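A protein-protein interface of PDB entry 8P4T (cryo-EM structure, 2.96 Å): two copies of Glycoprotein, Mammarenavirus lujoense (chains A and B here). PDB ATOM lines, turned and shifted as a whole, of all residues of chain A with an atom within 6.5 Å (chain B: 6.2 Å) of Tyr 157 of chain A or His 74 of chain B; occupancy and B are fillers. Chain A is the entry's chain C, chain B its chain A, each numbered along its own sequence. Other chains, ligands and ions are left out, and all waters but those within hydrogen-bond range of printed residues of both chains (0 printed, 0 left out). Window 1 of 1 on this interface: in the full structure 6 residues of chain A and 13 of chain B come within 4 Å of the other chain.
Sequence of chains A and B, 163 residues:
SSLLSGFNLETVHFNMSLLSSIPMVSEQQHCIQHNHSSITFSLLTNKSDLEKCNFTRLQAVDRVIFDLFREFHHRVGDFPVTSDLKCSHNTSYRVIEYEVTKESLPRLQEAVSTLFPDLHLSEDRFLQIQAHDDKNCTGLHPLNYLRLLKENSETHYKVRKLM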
ATOM      1  N   ASN A 152     -10.265   1.412 -30.780  1.00  0.00           N
ATOM      2  CA  ASN A 152     -10.157   0.065 -31.327  1.00  0.00           C
ATOM      3  C   ASN A 152      -8.704  -0.380 -31.399  1.00  0.00           C
ATOM      4  O   ASN A 152      -8.391  -1.547 -31.137  1.00  0.00           O
ATOM      5  CB  ASN A 152     -10.801   0.007 -32.711  1.00  0.00           C
ATOM      6  CG  ASN A 152     -12.258  -0.392 -32.656  1.00  0.00           C
ATOM      7  OD1 ASN A 152     -12.674  -1.133 -31.770  1.00  0.00           O
ATOM      8  ND2 ASN A 152     -13.042   0.094 -33.611  1.00  0.00           N
ATOM      9  N   GLU A 154      -6.057   0.771 -29.557  1.00  0.00           N
ATOM     10  CA  GLU A 154      -5.375   0.689 -28.269  1.00  0.00           C
ATOM     11  C   GLU A 154      -6.044  -0.249 -27.269  1.00  0.00           C
ATOM     12  O   GLU A 154      -5.348  -0.990 -26.566  1.00  0.00           O
ATOM     13  CB  GLU A 154      -5.258   2.083 -27.650  1.00  0.00           C
ATOM     14  CG  GLU A 154      -4.451   3.058 -28.481  1.00  0.00           C
ATOM     15  CD  GLU A 154      -2.992   2.665 -28.584  1.00  0.00           C
ATOM     16  OE1 GLU A 154      -2.441   2.150 -27.590  1.00  0.00           O
ATOM     17  OE2 GLU A 154      -2.395   2.872 -29.662  1.00  0.00           O
ATOM     18  N   THR A 155      -7.370  -0.240 -27.178  1.00  0.00           N
ATOM     19  CA  THR A 155      -8.076  -0.942 -26.112  1.00  0.00           C
ATOM     20  C   THR A 155      -8.935  -2.074 -26.683  1.00  0.00           C
ATOM     21  O   THR A 155     -10.058  -2.324 -26.241  1.00  0.00           O
ATOM     22  CB  THR A 155      -8.905   0.050 -25.295  1.00  0.00           C
ATOM     23  OG1 THR A 155      -8.064   1.138 -24.897  1.00  0.00           O
ATOM     24  CG2 THR A 155      -9.416  -0.583 -24.008  1.00  0.00           C
ATOM     25  N   HIS A 156      -8.424  -2.761 -27.707  1.00  0.00           N
ATOM     26  CA  HIS A 156      -9.136  -3.924 -28.227  1.00  0.00           C
ATOM     27  C   HIS A 156      -9.158  -5.074 -27.227  1.00  0.00           C
ATOM     28  O   HIS A 156     -10.120  -5.850 -27.199  1.00  0.00           O
ATOM     29  CB  HIS A 156      -8.515  -4.389 -29.542  1.00  0.00           C
ATOM     30  CG  HIS A 156      -9.212  -5.567 -30.150  1.00  0.00           C
ATOM     31  ND1 HIS A 156      -8.557  -6.736 -30.473  1.00  0.00           N
ATOM     32  CD2 HIS A 156     -10.511  -5.759 -30.482  1.00  0.00           C
ATOM     33  CE1 HIS A 156      -9.420  -7.594 -30.984  1.00  0.00           C
ATOM     34  NE2 HIS A 156     -10.613  -7.027 -31.001  1.00  0.00           N
ATOM     35  N   TYR A 157      -8.103  -5.218 -26.421  1.00  0.00           N
ATOM     36  CA  TYR A 157      -8.037  -6.322 -25.468  1.00  0.00           C
ATOM     37  C   TYR A 157      -9.165  -6.246 -24.444  1.00  0.00           C
ATOM     38  O   TYR A 157      -9.841  -7.246 -24.173  1.00  0.00           O
ATOM     39  CB  TYR A 157      -6.667  -6.347 -24.782  1.00  0.00           C
ATOM     40  CG  TYR A 157      -6.350  -5.142 -23.925  1.00  0.00           C
ATOM     41  CD1 TYR A 157      -5.963  -3.938 -24.498  1.00  0.00           C
ATOM     42  CD2 TYR A 157      -6.426  -5.212 -22.540  1.00  0.00           C
ATOM     43  CE1 TYR A 157      -5.670  -2.839 -23.717  1.00  0.00           C
ATOM     44  CE2 TYR A 157      -6.135  -4.119 -21.753  1.00  0.00           C
ATOM     45  CZ  TYR A 157      -5.757  -2.934 -22.346  1.00  0.00           C
ATOM     46  OH  TYR A 157      -5.464  -1.842 -21.563  1.00  0.00           O
ATOM     47  N   LYS A 158      -9.379  -5.065 -23.859  1.00  0.00           N
ATOM     48  CA  LYS A 158     -10.319  -4.929 -22.749  1.00  0.00           C
ATOM     49  C   LYS A 158     -11.759  -5.234 -23.152  1.00  0.00           C
ATOM     50  O   LYS A 158     -12.597  -5.470 -22.274  1.00  0.00           O
ATOM     51  CB  LYS A 158     -10.217  -3.519 -22.161  1.00  0.00           C
ATOM     52  CG  LYS A 158     -10.933  -3.330 -20.834  1.00  0.00           C
ATOM     53  CD  LYS A 158     -10.526  -2.034 -20.158  1.00  0.00           C
ATOM     54  CE  LYS A 158      -9.760  -2.305 -18.876  1.00  0.00           C
ATOM     55  NZ  LYS A 158      -9.826  -1.150 -17.939  1.00  0.00           N
ATOM     56  N   VAL A 159     -12.067  -5.262 -24.448  1.00  0.00           N
ATOM     57  CA  VAL A 159     -13.436  -5.467 -24.907  1.00  0.00           C
ATOM     58  C   VAL A 159     -13.653  -6.906 -25.373  1.00  0.00           C
ATOM     59  O   VAL A 159     -14.707  -7.231 -25.929  1.00  0.00           O
ATOM     60  CB  VAL A 159     -13.801  -4.453 -26.009  1.00  0.00           C
ATOM     61  CG1 VAL A 159     -13.064  -4.757 -27.307  1.00  0.00           C
ATOM     62  CG2 VAL A 159     -15.317  -4.337 -26.206  1.00  0.00           C
ATOM     63  N   ARG A 160     -12.684  -7.781 -25.135  1.00  0.00           N
ATOM     64  CA  ARG A 160     -12.775  -9.195 -25.462  1.00  0.00           C
ATOM     65  C   ARG A 160     -13.136  -9.991 -24.211  1.00  0.00           C
ATOM     66  O   ARG A 160     -12.878  -9.566 -23.082  1.00  0.00           O
ATOM     67  CB  ARG A 160     -11.446  -9.679 -26.054  1.00  0.00           C
ATOM     68  CG  ARG A 160     -11.393 -11.137 -26.476  1.00  0.00           C
ATOM     69  CD  ARG A 160     -10.045 -11.468 -27.102  1.00  0.00           C
ATOM     70  NE  ARG A 160      -9.597 -12.817 -26.776  1.00  0.00           N
ATOM     71  CZ  ARG A 160     -10.111 -13.926 -27.289  1.00  0.00           C
ATOM     72  NH1 ARG A 160     -11.095 -13.890 -28.172  1.00  0.00           N
ATOM     73  NH2 ARG A 160      -9.624 -15.103 -26.907  1.00  0.00           N
ATOM     74  N   LYS A 161     -13.749 -11.154 -24.426  1.00  0.00           N
ATOM     75  CA  LYS A 161     -14.225 -11.967 -23.313  1.00  0.00           C
ATOM     76  C   LYS A 161     -13.058 -12.445 -22.456  1.00  0.00           C
ATOM     77  O   LYS A 161     -11.958 -12.708 -22.949  1.00  0.00           O
ATOM     78  CB  LYS A 161     -15.033 -13.159 -23.828  1.00  0.00           C
ATOM     79  CG  LYS A 161     -14.221 -14.207 -24.570  1.00  0.00           C
ATOM     80  CD  LYS A 161     -15.116 -15.305 -25.121  1.00  0.00           C
ATOM     81  CE  LYS A 161     -14.306 -16.375 -25.833  1.00  0.00           C
ATOM     82  NZ  LYS A 161     -15.171 -17.466 -26.360  1.00  0.00           N
ATOM     83  N   LEU A 162     -13.307 -12.545 -21.153  1.00  0.00           N
ATOM     84  CA  LEU A 162     -12.268 -12.871 -20.185  1.00  0.00           C
ATOM     85  C   LEU A 162     -12.123 -14.368 -19.946  1.00  0.00           C
ATOM     86  O   LEU A 162     -11.234 -14.776 -19.192  1.00  0.00           O
ATOM     87  CB  LEU A 162     -12.546 -12.167 -18.852  1.00  0.00           C
ATOM     88  CG  LEU A 162     -12.251 -10.667 -18.773  1.00  0.00           C
ATOM     89  CD1 LEU A 162     -13.425  -9.845 -19.285  1.00  0.00           C
ATOM     90  CD2 LEU A 162     -11.892 -10.267 -17.352  1.00  0.00           C
ATOM     91  N   PHE B  69      -7.520  -6.837 -10.962  1.00  0.00           N
ATOM     92  CA  PHE B  69      -6.777  -7.883 -11.668  1.00  0.00           C
ATOM     93  C   PHE B  69      -7.040  -7.895 -13.169  1.00  0.00           C
ATOM     94  O   PHE B  69      -6.474  -8.751 -13.851  1.00  0.00           O
ATOM     95  CB  PHE B  69      -7.050  -9.330 -11.198  1.00  0.00           C
ATOM     96  CG  PHE B  69      -8.441  -9.836 -11.464  1.00  0.00           C
ATOM     97  CD1 PHE B  69      -9.471  -9.687 -10.573  1.00  0.00           C
ATOM     98  CD2 PHE B  69      -8.685 -10.540 -12.639  1.00  0.00           C
ATOM     99  CE1 PHE B  69     -10.726 -10.176 -10.867  1.00  0.00           C
ATOM    100  CE2 PHE B  69      -9.931 -11.036 -12.930  1.00  0.00           C
ATOM    101  CZ  PHE B  69     -10.951 -10.859 -12.041  1.00  0.00           C
ATOM    102  N   ARG B  70      -7.928  -7.042 -13.694  1.00  0.00           N
ATOM    103  CA  ARG B  70      -8.314  -7.175 -15.100  1.00  0.00           C
ATOM    104  C   ARG B  70      -7.132  -6.986 -16.047  1.00  0.00           C
ATOM    105  O   ARG B  70      -6.982  -7.742 -17.017  1.00  0.00           O
ATOM    106  CB  ARG B  70      -9.436  -6.193 -15.436  1.00  0.00           C
ATOM    107  CG  ARG B  70     -10.366  -6.693 -16.536  1.00  0.00           C
ATOM    108  CD  ARG B  70     -11.332  -5.618 -17.005  1.00  0.00           C
ATOM    109  NE  ARG B  70     -12.082  -6.045 -18.181  1.00  0.00           N
ATOM    110  CZ  ARG B  70     -13.039  -5.333 -18.760  1.00  0.00           C
ATOM    111  NH1 ARG B  70     -13.391  -4.143 -18.299  1.00  0.00           N
ATOM    112  NH2 ARG B  70     -13.663  -5.829 -19.824  1.00  0.00           N
ATOM    113  N   GLU B  71      -6.293  -5.978 -15.805  1.00  0.00           N
ATOM    114  CA  GLU B  71      -5.138  -5.772 -16.675  1.00  0.00           C
ATOM    115  C   GLU B  71      -4.168  -6.946 -16.598  1.00  0.00           C
ATOM    116  O   GLU B  71      -3.634  -7.384 -17.625  1.00  0.00           O
ATOM    117  CB  GLU B  71      -4.440  -4.463 -16.314  1.00  0.00           C
ATOM    118  CG  GLU B  71      -5.257  -3.235 -16.663  1.00  0.00           C
ATOM    119  CD  GLU B  71      -5.351  -3.008 -18.158  1.00  0.00           C
ATOM    120  OE1 GLU B  71      -4.385  -3.342 -18.876  1.00  0.00           O
ATOM    121  OE2 GLU B  71      -6.397  -2.507 -18.618  1.00  0.00           O
ATOM    122  N   PHE B  72      -3.933  -7.480 -15.396  1.00  0.00           N
ATOM    123  CA  PHE B  72      -3.064  -8.647 -15.272  1.00  0.00           C
ATOM    124  C   PHE B  72      -3.647  -9.841 -16.019  1.00  0.00           C
ATOM    125  O   PHE B  72      -2.915 -10.598 -16.669  1.00  0.00           O
ATOM    126  CB  PHE B  72      -2.848  -8.989 -13.798  1.00  0.00           C
ATOM    127  CG  PHE B  72      -2.287 -10.365 -13.569  1.00  0.00           C
ATOM    128  CD1 PHE B  72      -0.936 -10.614 -13.739  1.00  0.00           C
ATOM    129  CD2 PHE B  72      -3.111 -11.410 -13.183  1.00  0.00           C
ATOM    130  CE1 PHE B  72      -0.417 -11.877 -13.530  1.00  0.00           C
ATOM    131  CE2 PHE B  72      -2.598 -12.675 -12.975  1.00  0.00           C
ATOM    132  CZ  PHE B  72      -1.249 -12.907 -13.149  1.00  0.00           C
ATOM    133  N   HIS B  73      -4.966 -10.024 -15.936  1.00  0.00           N
ATOM    134  CA  HIS B  73      -5.606 -11.164 -16.584  1.00  0.00           C
ATOM    135  C   HIS B  73      -5.513 -11.044 -18.097  1.00  0.00           C
ATOM    136  O   HIS B  73      -5.297 -12.041 -18.796  1.00  0.00           O
ATOM    137  CB  HIS B  73      -7.064 -11.276 -16.140  1.00  0.00           C
ATOM    138  CG  HIS B  73      -7.787 -12.449 -16.728  1.00  0.00           C
ATOM    139  ND1 HIS B  73      -7.439 -13.753 -16.448  1.00  0.00           N
ATOM    140  CD2 HIS B  73      -8.839 -12.514 -17.577  1.00  0.00           C
ATOM    141  CE1 HIS B  73      -8.245 -14.571 -17.102  1.00  0.00           C
ATOM    142  NE2 HIS B  73      -9.104 -13.845 -17.794  1.00  0.00           N
ATOM    143  N   HIS B  74      -5.680  -9.827 -18.621  1.00  0.00           N
ATOM    144  CA  HIS B  74      -5.525  -9.622 -20.056  1.00  0.00           C
ATOM    145  C   HIS B  74      -4.071  -9.768 -20.484  1.00  0.00           C
ATOM    146  O   HIS B  74      -3.797 -10.127 -21.634  1.00  0.00           O
ATOM    147  CB  HIS B  74      -6.058  -8.245 -20.448  1.00  0.00           C
ATOM    148  CG  HIS B  74      -7.552  -8.141 -20.418  1.00  0.00           C
ATOM    149  ND1 HIS B  74      -8.373  -9.025 -21.084  1.00  0.00           N
ATOM    150  CD2 HIS B  74      -8.371  -7.259 -19.801  1.00  0.00           C
ATOM    151  CE1 HIS B  74      -9.634  -8.691 -20.879  1.00  0.00           C
ATOM    152  NE2 HIS B  74      -9.660  -7.622 -20.103  1.00  0.00           N
ATOM    153  N   ARG B  75      -3.128  -9.494 -19.576  1.00  0.00           N
ATOM    154  CA  ARG B  75      -1.723  -9.757 -19.869  1.00  0.00           C
ATOM    155  C   ARG B  75      -1.412 -11.248 -19.859  1.00  0.00           C
ATOM    156  O   ARG B  75      -0.484 -11.691 -20.545  1.00  0.00           O
ATOM    157  CB  ARG B  75      -0.834  -9.024 -18.865  1.00  0.00           C
ATOM    158  CG  ARG B  75       0.649  -9.034 -19.208  1.00  0.00           C
ATOM    159  CD  ARG B  75       0.892  -8.730 -20.677  1.00  0.00           C
ATOM    160  NE  ARG B  75       2.315  -8.661 -20.985  1.00  0.00           N
ATOM    161  CZ  ARG B  75       3.031  -9.675 -21.451  1.00  0.00           C
ATOM    162  NH1 ARG B  75       2.486 -10.857 -21.681  1.00  0.00           N
ATOM    163  NH2 ARG B  75       4.327  -9.499 -21.690  1.00  0.00           N
ATOM    164  N   VAL B  76      -2.175 -12.037 -19.099  1.00  0.00           N
ATOM    165  CA  VAL B  76      -2.028 -13.488 -19.167  1.00  0.00           C
ATOM    166  C   VAL B  76      -2.525 -14.018 -20.508  1.00  0.00           C
ATOM    167  O   VAL B  76      -1.995 -15.006 -21.030  1.00  0.00           O
ATOM    168  CB  VAL B  76      -2.755 -14.153 -17.982  1.00  0.00           C
ATOM    169  CG1 VAL B  76      -2.733 -15.668 -18.110  1.00  0.00           C
ATOM    170  CG2 VAL B  76      -2.123 -13.726 -16.670  1.00  0.00           C
ATOM    171  N   GLY B  77      -3.516 -13.360 -21.102  1.00  0.00           N
ATOM    172  CA  GLY B  77      -4.004 -13.756 -22.408  1.00  0.00           C
ATOM    173  C   GLY B  77      -4.943 -14.942 -22.375  1.00  0.00           C
ATOM    174  O   GLY B  77      -5.778 -15.057 -21.473  1.00  0.00           O
ATOM    175  N   ASP B  78      -4.818 -15.833 -23.357  1.00  0.00           N
ATOM    176  CA  ASP B  78      -5.686 -17.005 -23.456  1.00  0.00           C
ATOM    177  C   ASP B  78      -5.226 -18.048 -22.446  1.00  0.00           C
ATOM    178  O   ASP B  78      -4.314 -18.834 -22.713  1.00  0.00           O
ATOM    179  CB  ASP B  78      -5.669 -17.561 -24.874  1.00  0.00           C
ATOM    180  CG  ASP B  78      -6.542 -16.764 -25.823  1.00  0.00           C
ATOM    181  OD1 ASP B  78      -6.989 -15.664 -25.438  1.00  0.00           O
ATOM    182  OD2 ASP B  78      -6.781 -17.236 -26.953  1.00  0.00           O
ATOM    183  N   LEU B 148       2.509  -2.555 -17.700  1.00  0.00           N
ATOM    184  CA  LEU B 148       1.478  -3.554 -17.963  1.00  0.00           C
ATOM    185  C   LEU B 148       0.454  -3.031 -18.960  1.00  0.00           C
ATOM    186  O   LEU B 148       0.069  -3.739 -19.899  1.00  0.00           O
ATOM    187  CB  LEU B 148       0.799  -3.953 -16.653  1.00  0.00           C
ATOM    188  CG  LEU B 148      -0.082  -5.201 -16.655  1.00  0.00           C
ATOM    189  CD1 LEU B 148       0.775  -6.450 -16.705  1.00  0.00           C
ATOM    190  CD2 LEU B 148      -0.975  -5.216 -15.428  1.00  0.00           C
ATOM    191  N   LEU B 149       0.014  -1.783 -18.781  1.00  0.00           N
ATOM    192  CA  LEU B 149      -0.978  -1.206 -19.684  1.00  0.00           C
ATOM    193  C   LEU B 149      -0.424  -1.081 -21.096  1.00  0.00           C
ATOM    194  O   LEU B 149      -1.118  -1.381 -22.076  1.00  0.00           O
ATOM    195  CB  LEU B 149      -1.429   0.160 -19.170  1.00  0.00           C
ATOM    196  CG  LEU B 149      -2.207   0.231 -17.856  1.00  0.00           C
ATOM    197  CD1 LEU B 149      -1.992   1.580 -17.195  1.00  0.00           C
ATOM    198  CD2 LEU B 149      -3.683  -0.009 -18.099  1.00  0.00           C
ATOM    199  N   ASN B 152      -0.177  -4.460 -22.709  1.00  0.00           N
ATOM    200  CA  ASN B 152      -1.502  -4.942 -23.079  1.00  0.00           C
ATOM    201  C   ASN B 152      -2.004  -4.251 -24.337  1.00  0.00           C
ATOM    202  O   ASN B 152      -2.639  -4.883 -25.189  1.00  0.00           O
ATOM    203  CB  ASN B 152      -2.480  -4.726 -21.925  1.00  0.00           C
ATOM    204  CG  ASN B 152      -2.567  -5.920 -21.004  1.00  0.00           C
ATOM    205  OD1 ASN B 152      -2.385  -7.058 -21.431  1.00  0.00           O
ATOM    206  ND2 ASN B 152      -2.849  -5.669 -19.732  1.00  0.00           N
ATOM    207  N   SER B 153      -1.731  -2.953 -24.471  1.00  0.00           N
ATOM    208  CA  SER B 153      -2.232  -2.214 -25.624  1.00  0.00           C
ATOM    209  C   SER B 153      -1.469  -2.569 -26.895  1.00  0.00           C
ATOM    210  O   SER B 153      -2.066  -2.681 -27.971  1.00  0.00           O
ATOM    211  CB  SER B 153      -2.154  -0.710 -25.358  1.00  0.00           C
ATOM    212  OG  SER B 153      -2.994  -0.340 -24.280  1.00  0.00           O
ATOM    213  N   HIS B 156      -0.974  -7.279 -27.363  1.00  0.00           N
ATOM    214  CA  HIS B 156      -2.072  -8.188 -27.042  1.00  0.00           C
ATOM    215  C   HIS B 156      -2.127  -9.375 -27.997  1.00  0.00           C
ATOM    216  O   HIS B 156      -2.537 -10.470 -27.595  1.00  0.00           O
ATOM    217  CB  HIS B 156      -3.405  -7.444 -27.060  1.00  0.00           C
ATOM    218  CG  HIS B 156      -4.577  -8.308 -26.713  1.00  0.00           C
ATOM    219  ND1 HIS B 156      -5.672  -8.443 -27.538  1.00  0.00           N
ATOM    220  CD2 HIS B 156      -4.818  -9.093 -25.636  1.00  0.00           C
ATOM    221  CE1 HIS B 156      -6.542  -9.267 -26.981  1.00  0.00           C
ATOM    222  NE2 HIS B 156      -6.047  -9.675 -25.826  1.00  0.00           N
ATOM    223  N   VAL B 159       0.055 -12.670 -27.224  1.00  0.00           N
ATOM    224  CA  VAL B 159      -0.280 -13.447 -26.036  1.00  0.00           C
ATOM    225  C   VAL B 159      -1.576 -14.232 -26.235  1.00  0.00           C
ATOM    226  O   VAL B 159      -2.094 -14.833 -25.289  1.00  0.00           O
ATOM    227  CB  VAL B 159      -0.351 -12.539 -24.791  1.00  0.00           C
ATOM    228  CG1 VAL B 159      -1.574 -11.633 -24.839  1.00  0.00           C
ATOM    229  CG2 VAL B 159      -0.263 -13.340 -23.488  1.00  0.00           C
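NH2 of Arg 70 of chain B is in hydrogen-bond range of O of Lys 158 of chain A, 2.7 Å away. The side-chain carboxylate (OE2) of Glu 71 of chain B sits at hydrogen-bond distance from the side-chain hydroxyl (OH) of Tyr 157 of chain A. OE2 of Glu 71 of chain B is in salt-bridge range of NZ of Lys 158 of chain A. NE2 of His 73 of chain B sits at hydrogen-bond distance from O of Leu 162 of chain A (2.7 Å). The side-chain carboxylate (OD1) of Asp 78 of chain B lies within salt-bridge range of the guanidinium group (NH2) of Arg 160 of chain A, 3.1 Å away. The side-chain hydroxyl (OG) of Ser 153 of chain B lies within hydrogen-bond range of the backbone carbonyl oxygen (O) of Glu 154 of chain A.
The guanidinium group of Arg 70 of chain B lies within hydrogen-bond range of a ring nitrogen (NE2) of His 74 of chain B (3.5 Å). The side-chain amide nitrogen (ND2) of Asn 152 of chain B sits at hydrogen-bond distance from the backbone carbonyl oxygen (O) of Glu 71 of chain B, at 2.8 Å. The backbone carbonyl oxygen of His 74 of chain B lies close to the side-chain amide oxygen of Asn 152 of chain B, 3.4 Å away. The side-chain amide oxygen (OD1) of Asn 152 of chain B is in hydrogen-bond range of the backbone NH (N) of Arg 75 of chain B (3.2 Å). The backbone carbonyl oxygen of Val 159 of chain B lies within hydrogen-bond range of the backbone NH of Asp 78 of chain B (3.5 Å). The backbone carbonyl oxygen of Leu 149 of chain B sits at hydrogen-bond distance from the side-chain hydroxyl of Ser 153 of chain B (3.1 Å).
CE1 of His 74 of chain B touches O of Tyr 157 of chain A (3.6 Å). Tyr 157 of chain A touches Asn 152 of chain B. Ser 153 of chain B touches Tyr 157 of chain A (OG to CE1, 3.7 Å). Tyr 157 of chain A touches His 156 of chain B (CB to CD2, 3.4 Å). Lys 158 of chain A touches His 74 of chain B. CD2 of Leu 162 of chain A touches CG of Arg 70 of chain B, at 3.97 Å. Leu 162 of chain A touches His 74 of chain B.
Tyr 157 of chain A touches just these residues of chain B: Glu 71, His 74, Asn 152, Ser 153 and His 156. Of the printed residues of chain A, His 74 of chain B touches Tyr 157, Lys 158 and Leu 162. Of the printed residues of chain B, Glu 154 of chain A touches Ser 153. Printed residues of chain A within 4 Å of Ser 153 of chain B: Glu 154 (3.3 Å) and Tyr 157 (3.7 Å). Of the printed residues of chain A, Asn 152 of chain B touches Tyr 157 (3.5 Å). Printed residues of chain A within 4 Å of Asp 78 of chain B: Arg 160 (3.1 Å). The nearest printed residue of chain A that does not touch His 74 of chain B is Arg 160 of chain A (4.02 Å).
Of the 10 printed residues of chain A, 5 touch a printed residue of chain B. Printed residues of chain A that touch a printed residue of chain B: Glu 154, Tyr 157, Lys 158, Arg 160 and Leu 162. Hydrophobic or aromatic side chains of chain A that line the printed part of chain B: Tyr 157 and Leu 162. Along chain A the printed residues that touch a printed residue of chain B span positions 154 to 162. Printed residues of chain B that touch a printed residue of chain A: Arg 70, Glu 71, His 73, His 74, Asp 78, Asn 152, Ser 153 and His 156. Hydrophobic or aromatic side chains of chain B within 4 Å of the printed part of chain A: His 73, His 74 and His 156. Along chain B the printed residues that touch a printed residue of chain A span positions 70 to 156. Among the printed residues, 13 pairs touch across the chains. Among the printed residues, Asp or Glu carboxylates within 4 Å of a Lys or Arg side-chain nitrogen of the other chain: Lys 158 of chain A with Glu 71 of chain B (3.7 Å) and Arg 160 of chain A with Asp 78 of chain B (3.1 Å).
3 positions are printed for both chains.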
